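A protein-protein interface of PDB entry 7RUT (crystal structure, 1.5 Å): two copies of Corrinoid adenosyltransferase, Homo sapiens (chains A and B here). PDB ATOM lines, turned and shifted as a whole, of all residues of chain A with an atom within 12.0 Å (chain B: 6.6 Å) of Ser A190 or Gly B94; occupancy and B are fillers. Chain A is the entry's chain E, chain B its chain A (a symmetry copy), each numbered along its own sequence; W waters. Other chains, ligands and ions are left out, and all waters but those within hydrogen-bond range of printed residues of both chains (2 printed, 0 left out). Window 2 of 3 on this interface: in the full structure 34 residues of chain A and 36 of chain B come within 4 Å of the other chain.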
ATOM      1  N   MET A 185     -28.375  -9.680 -17.712  1.00  0.00           N
ATOM      2  CA  MET A 185     -28.213  -9.707 -16.267  1.00  0.00           C
ATOM      3  C   MET A 185     -26.727  -9.621 -15.963  1.00  0.00           C
ATOM      4  O   MET A 185     -25.920 -10.247 -16.653  1.00  0.00           O
ATOM      5  CB  MET A 185     -28.815 -10.981 -15.655  1.00  0.00           C
ATOM      6  N   LYS A 186     -26.364  -8.836 -14.950  1.00  0.00           N
ATOM      7  CA  LYS A 186     -24.957  -8.669 -14.616  1.00  0.00           C
ATOM      8  C   LYS A 186     -24.339 -10.000 -14.205  1.00  0.00           C
ATOM      9  O   LYS A 186     -24.846 -10.681 -13.308  1.00  0.00           O
ATOM     10  CB  LYS A 186     -24.802  -7.637 -13.496  1.00  0.00           C
ATOM     11  CG  LYS A 186     -23.354  -7.316 -13.155  1.00  0.00           C
ATOM     12  CD  LYS A 186     -22.687  -6.499 -14.256  1.00  0.00           C
ATOM     13  CE  LYS A 186     -21.264  -6.978 -14.505  1.00  0.00           C
ATOM     14  NZ  LYS A 186     -20.354  -5.864 -14.911  1.00  0.00           N
ATOM     15  N   ASN A 187     -23.249 -10.373 -14.878  1.00  0.00           N
ATOM     16  CA  ASN A 187     -22.485 -11.577 -14.566  1.00  0.00           C
ATOM     17  C   ASN A 187     -21.240 -11.151 -13.799  1.00  0.00           C
ATOM     18  O   ASN A 187     -20.334 -10.530 -14.368  1.00  0.00           O
ATOM     19  CB  ASN A 187     -22.113 -12.334 -15.841  1.00  0.00           C
ATOM     20  CG  ASN A 187     -21.427 -13.658 -15.555  1.00  0.00           C
ATOM     21  OD1 ASN A 187     -21.808 -14.379 -14.633  1.00  0.00           O
ATOM     22  ND2 ASN A 187     -20.408 -13.982 -16.345  1.00  0.00           N
ATOM     23  N   ASP A 188     -21.192 -11.482 -12.511  1.00  0.00           N
ATOM     24  CA  ASP A 188     -20.145 -10.990 -11.611  1.00  0.00           C
ATOM     25  C   ASP A 188     -19.668 -12.131 -10.722  1.00  0.00           C
ATOM     26  O   ASP A 188     -19.867 -12.119  -9.499  1.00  0.00           O
ATOM     27  CB  ASP A 188     -20.664  -9.814 -10.780  1.00  0.00           C
ATOM     28  CG  ASP A 188     -19.578  -9.153  -9.959  1.00  0.00           C
ATOM     29  OD1 ASP A 188     -18.378  -9.345 -10.269  1.00  0.00           O
ATOM     30  OD2 ASP A 188     -19.934  -8.437  -8.999  1.00  0.00           O
ATOM     31  N   PRO A 189     -19.002 -13.133 -11.310  1.00  0.00           N
ATOM     32  CA  PRO A 189     -18.644 -14.330 -10.533  1.00  0.00           C
ATOM     33  C   PRO A 189     -17.660 -14.067  -9.406  1.00  0.00           C
ATOM     34  O   PRO A 189     -17.607 -14.863  -8.461  1.00  0.00           O
ATOM     35  CB  PRO A 189     -18.039 -15.268 -11.587  1.00  0.00           C
ATOM     36  CG  PRO A 189     -17.569 -14.351 -12.686  1.00  0.00           C
ATOM     37  CD  PRO A 189     -18.565 -13.231 -12.716  1.00  0.00           C
ATOM     38  N   SER A 190     -16.885 -12.989  -9.467  1.00  0.00           N
ATOM     39  CA  SER A 190     -15.901 -12.699  -8.433  1.00  0.00           C
ATOM     40  C   SER A 190     -16.325 -11.553  -7.525  1.00  0.00           C
ATOM     41  O   SER A 190     -15.506 -11.078  -6.737  1.00  0.00           O
ATOM     42  CB  SER A 190     -14.538 -12.393  -9.061  1.00  0.00           C
ATOM     43  OG  SER A 190     -13.876 -13.582  -9.469  1.00  0.00           O
ATOM     44  N   ALA A 191     -17.581 -11.109  -7.606  1.00  0.00           N
ATOM     45  CA  ALA A 191     -18.102 -10.049  -6.737  1.00  0.00           C
ATOM     46  C   ALA A 191     -17.225  -8.797  -6.808  1.00  0.00           C
ATOM     47  O   ALA A 191     -16.814  -8.225  -5.790  1.00  0.00           O
ATOM     48  CB  ALA A 191     -18.244 -10.549  -5.299  1.00  0.00           C
ATOM     49  N   GLU A 192     -16.936  -8.374  -8.041  1.00  0.00           N
ATOM     50  CA  GLU A 192     -16.100  -7.205  -8.297  1.00  0.00           C
ATOM     51  C   GLU A 192     -16.891  -5.970  -8.695  1.00  0.00           C
ATOM     52  O   GLU A 192     -16.331  -4.868  -8.688  1.00  0.00           O
ATOM     53  CB  GLU A 192     -15.086  -7.511  -9.407  1.00  0.00           C
ATOM     54  CG  GLU A 192     -14.309  -8.787  -9.197  1.00  0.00           C
ATOM     55  CD  GLU A 192     -13.482  -9.176 -10.409  1.00  0.00           C
ATOM     56  OE1 GLU A 192     -12.252  -8.980 -10.369  1.00  0.00           O
ATOM     57  OE2 GLU A 192     -14.062  -9.676 -11.398  1.00  0.00           O
ATOM     58  N   SER A 193     -18.160  -6.122  -9.059  1.00  0.00           N
ATOM     59  CA  SER A 193     -18.963  -4.975  -9.452  1.00  0.00           C
ATOM     60  C   SER A 193     -19.186  -4.047  -8.268  1.00  0.00           C
ATOM     61  O   SER A 193     -19.367  -4.490  -7.131  1.00  0.00           O
ATOM     62  CB  SER A 193     -20.308  -5.427 -10.017  1.00  0.00           C
ATOM     63  OG  SER A 193     -20.924  -4.377 -10.741  1.00  0.00           O
ATOM     64  N   GLU A 194     -19.165  -2.748  -8.542  1.00  0.00           N
ATOM     65  CA  GLU A 194     -19.454  -1.739  -7.533  1.00  0.00           C
ATOM     66  C   GLU A 194     -20.847  -1.149  -7.687  1.00  0.00           C
ATOM     67  O   GLU A 194     -21.517  -0.884  -6.685  1.00  0.00           O
ATOM     68  CB  GLU A 194     -18.406  -0.623  -7.597  1.00  0.00           C
ATOM     69  CG  GLU A 194     -16.997  -1.137  -7.843  1.00  0.00           C
ATOM     70  CD  GLU A 194     -15.931  -0.211  -7.299  1.00  0.00           C
ATOM     71  OE1 GLU A 194     -16.206   1.001  -7.173  1.00  0.00           O
ATOM     72  OE2 GLU A 194     -14.822  -0.700  -6.988  1.00  0.00           O
ATOM     73  N   GLY A 195     -21.301  -0.957  -8.923  1.00  0.00           N
ATOM     74  CA  GLY A 195     -22.621  -0.417  -9.186  1.00  0.00           C
ATOM     75  C   GLY A 195     -22.935  -0.359 -10.667  1.00  0.00           C
ATOM     76  O   GLY A 195     -23.688   0.504 -11.118  1.00  0.00           O
ATOM     77  N   PHE B  91     -13.099  -3.340 -17.031  1.00  0.00           N
ATOM     78  CA  PHE B  91     -13.611  -4.673 -17.294  1.00  0.00           C
ATOM     79  C   PHE B  91     -12.927  -5.620 -16.317  1.00  0.00           C
ATOM     80  O   PHE B  91     -11.721  -5.868 -16.428  1.00  0.00           O
ATOM     81  CB  PHE B  91     -13.357  -5.064 -18.744  1.00  0.00           C
ATOM     82  CG  PHE B  91     -13.943  -6.372 -19.116  1.00  0.00           C
ATOM     83  CD1 PHE B  91     -13.208  -7.536 -18.973  1.00  0.00           C
ATOM     84  CD2 PHE B  91     -15.234  -6.446 -19.607  1.00  0.00           C
ATOM     85  CE1 PHE B  91     -13.748  -8.751 -19.311  1.00  0.00           C
ATOM     86  CE2 PHE B  91     -15.781  -7.664 -19.952  1.00  0.00           C
ATOM     87  CZ  PHE B  91     -15.037  -8.818 -19.801  1.00  0.00           C
ATOM     88  N   LYS B  92     -13.695  -6.144 -15.364  1.00  0.00           N
ATOM     89  CA  LYS B  92     -13.143  -6.981 -14.310  1.00  0.00           C
ATOM     90  C   LYS B  92     -12.805  -8.370 -14.841  1.00  0.00           C
ATOM     91  O   LYS B  92     -13.424  -8.860 -15.787  1.00  0.00           O
ATOM     92  CB  LYS B  92     -14.130  -7.089 -13.149  1.00  0.00           C
ATOM     93  CG  LYS B  92     -14.507  -5.750 -12.545  1.00  0.00           C
ATOM     94  CD  LYS B  92     -13.297  -5.068 -11.925  1.00  0.00           C
ATOM     95  CE  LYS B  92     -13.688  -3.790 -11.202  1.00  0.00           C
ATOM     96  NZ  LYS B  92     -12.488  -3.107 -10.653  1.00  0.00           N
ATOM     97  N   ALA B  93     -11.811  -9.004 -14.215  1.00  0.00           N
ATOM     98  CA  ALA B  93     -11.257 -10.255 -14.722  1.00  0.00           C
ATOM     99  C   ALA B  93     -12.007 -11.502 -14.263  1.00  0.00           C
ATOM    100  O   ALA B  93     -11.708 -12.596 -14.758  1.00  0.00           O
ATOM    101  CB  ALA B  93      -9.784 -10.381 -14.314  1.00  0.00           C
ATOM    102  N   GLY B  94     -12.961 -11.373 -13.338  1.00  0.00           N
ATOM    103  CA  GLY B  94     -13.725 -12.504 -12.850  1.00  0.00           C
ATOM    104  C   GLY B  94     -14.201 -13.486 -13.911  1.00  0.00           C
ATOM    105  O   GLY B  94     -14.020 -14.700 -13.773  1.00  0.00           O
ATOM    106  N   PRO B  95     -14.832 -12.990 -14.982  1.00  0.00           N
ATOM    107  CA  PRO B  95     -15.301 -13.901 -16.039  1.00  0.00           C
ATOM    108  C   PRO B  95     -14.189 -14.673 -16.726  1.00  0.00           C
ATOM    109  O   PRO B  95     -14.437 -15.780 -17.225  1.00  0.00           O
ATOM    110  CB  PRO B  95     -16.021 -12.959 -17.012  1.00  0.00           C
ATOM    111  CG  PRO B  95     -16.528 -11.859 -16.121  1.00  0.00           C
ATOM    112  CD  PRO B  95     -15.405 -11.637 -15.136  1.00  0.00           C
ATOM    113  N   ILE B  96     -12.973 -14.131 -16.781  1.00  0.00           N
ATOM    114  CA  ILE B  96     -11.861 -14.867 -17.380  1.00  0.00           C
ATOM    115  C   ILE B  96     -11.549 -16.102 -16.548  1.00  0.00           C
ATOM    116  O   ILE B  96     -11.363 -17.204 -17.077  1.00  0.00           O
ATOM    117  CB  ILE B  96     -10.623 -13.964 -17.514  1.00  0.00           C
ATOM    118  CG1 ILE B  96     -10.956 -12.689 -18.298  1.00  0.00           C
ATOM    119  CG2 ILE B  96      -9.491 -14.732 -18.182  1.00  0.00           C
ATOM    120  CD1 ILE B  96      -9.891 -11.597 -18.159  1.00  0.00           C
ATOM    121  N   LEU B  97     -11.497 -15.934 -15.223  1.00  0.00           N
ATOM    122  CA  LEU B  97     -11.221 -17.064 -14.343  1.00  0.00           C
ATOM    123  C   LEU B  97     -12.322 -18.113 -14.431  1.00  0.00           C
ATOM    124  O   LEU B  97     -12.048 -19.319 -14.387  1.00  0.00           O
ATOM    125  CB  LEU B  97     -11.058 -16.579 -12.904  1.00  0.00           C
ATOM    126  CG  LEU B  97      -9.801 -15.751 -12.636  1.00  0.00           C
ATOM    127  CD1 LEU B  97      -9.941 -14.960 -11.343  1.00  0.00           C
ATOM    128  CD2 LEU B  97      -8.574 -16.648 -12.588  1.00  0.00           C
ATOM    129  N   GLU B  98     -13.575 -17.674 -14.559  1.00  0.00           N
ATOM    130  CA  GLU B  98     -14.666 -18.633 -14.675  1.00  0.00           C
ATOM    131  C   GLU B  98     -14.566 -19.430 -15.973  1.00  0.00           C
ATOM    132  O   GLU B  98     -14.840 -20.638 -15.985  1.00  0.00           O
ATOM    133  CB  GLU B  98     -16.021 -17.933 -14.569  1.00  0.00           C
ATOM    134  CG  GLU B  98     -17.155 -18.943 -14.369  1.00  0.00           C
ATOM    135  CD  GLU B  98     -18.475 -18.314 -13.951  1.00  0.00           C
ATOM    136  OE1 GLU B  98     -18.837 -17.253 -14.497  1.00  0.00           O
ATOM    137  OE2 GLU B  98     -19.157 -18.895 -13.077  1.00  0.00           O
ATOM    138  N   LEU B  99     -14.165 -18.784 -17.073  1.00  0.00           N
ATOM    139  CA  LEU B  99     -13.931 -19.524 -18.311  1.00  0.00           C
ATOM    140  C   LEU B  99     -12.859 -20.586 -18.122  1.00  0.00           C
ATOM    141  O   LEU B  99     -12.993 -21.702 -18.632  1.00  0.00           O
ATOM    142  CB  LEU B  99     -13.526 -18.582 -19.442  1.00  0.00           C
ATOM    143  CG  LEU B  99     -14.578 -17.692 -20.083  1.00  0.00           C
ATOM    144  CD1 LEU B  99     -13.918 -16.864 -21.192  1.00  0.00           C
ATOM    145  CD2 LEU B  99     -15.763 -18.480 -20.633  1.00  0.00           C
ATOM    146  N   GLN B 101     -12.066 -22.149 -15.353  1.00  0.00           N
ATOM    147  CA  GLN B 101     -12.638 -23.234 -14.563  1.00  0.00           C
ATOM    148  C   GLN B 101     -13.533 -24.127 -15.417  1.00  0.00           C
ATOM    149  O   GLN B 101     -13.511 -25.360 -15.274  1.00  0.00           O
ATOM    150  CB  GLN B 101     -13.403 -22.649 -13.371  1.00  0.00           C
ATOM    151  CG  GLN B 101     -12.496 -21.842 -12.440  1.00  0.00           C
ATOM    152  CD  GLN B 101     -13.235 -21.058 -11.375  1.00  0.00           C
ATOM    153  OE1 GLN B 101     -12.700 -20.819 -10.294  1.00  0.00           O
ATOM    154  NE2 GLN B 101     -14.456 -20.642 -11.675  1.00  0.00           N
HETATM  155  O   HOH W   1     -14.687 -15.671 -11.203  1.00  0.00           O
HETATM  156  O   HOH W   2     -21.267 -16.521 -13.322  1.00  0.00           O
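N of Gly B94 sits at hydrogen-bond distance from OE2 of Glu A192 (2.8 Å).
The side-chain carboxylate (OD1) of Asp A188 sits at hydrogen-bond distance from the backbone NH (N) of Glu A192 (2.8 Å).
Gly B94 touches Pro A189. N of Pro B95 touches CG of Pro A189, 3.8 Å away. CB of Pro A189 touches OE1 of Glu B98, at 3.6 Å. Ser A190 touches Gly B94. Lys B92 touches Glu A192 (CB to OE2, 3.1 Å). OE2 of Glu A192 touches N of Ala B93 (3.7 Å).
Of chain B, only Gly B94 (3.6 Å) comes within 4 Å of Ser A190. Of chain A, only Pro A189 (3.7 Å), Ser A190 (3.6 Å) and Glu A192 (2.8 Å) come within 4 Å of Gly B94. Of the printed residues of chain A, Ala B93 touches Glu A192. Pro B95 touches just one residue of chain A: Pro A189 (3.8 Å). No residue of chain A comes within 4 Å of Ile B96. Printed residues of chain A within 4 Å of Glu B98: Pro A189 (3.6 Å). Printed residues of chain B within 4 Å of Pro A189: Gly B94 (3.7 Å), Pro B95 (3.8 Å) and Glu B98 (3.6 Å). Of the printed residues of chain B, Glu A192 touches Lys B92 (3.1 Å), Ala B93 (3.7 Å) and Gly B94 (2.8 Å). Printed residues of chain A within 4 Å of Lys B92: Glu A192. Lys A186 touches none of the printed residues of chain B.
Printed residues of chain A that touch a printed residue of chain B: Pro A189, Ser A190 and Glu A192. Along chain A the printed residues that touch a printed residue of chain B span positions 189 to 192. Among the printed residues, no Asp or Glu carboxylate lies within 4 Å of a Lys or Arg side-chain nitrogen of the other chain.
No position is printed for both chains.
Water W2 lies within hydrogen-bond range of OD1 of Asn A187 (2.6 Å) and OE1 of Glu B98 (2.8 Å). Water W1 lies within hydrogen-bond range of O of Gly B94 and OG of Ser A190.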
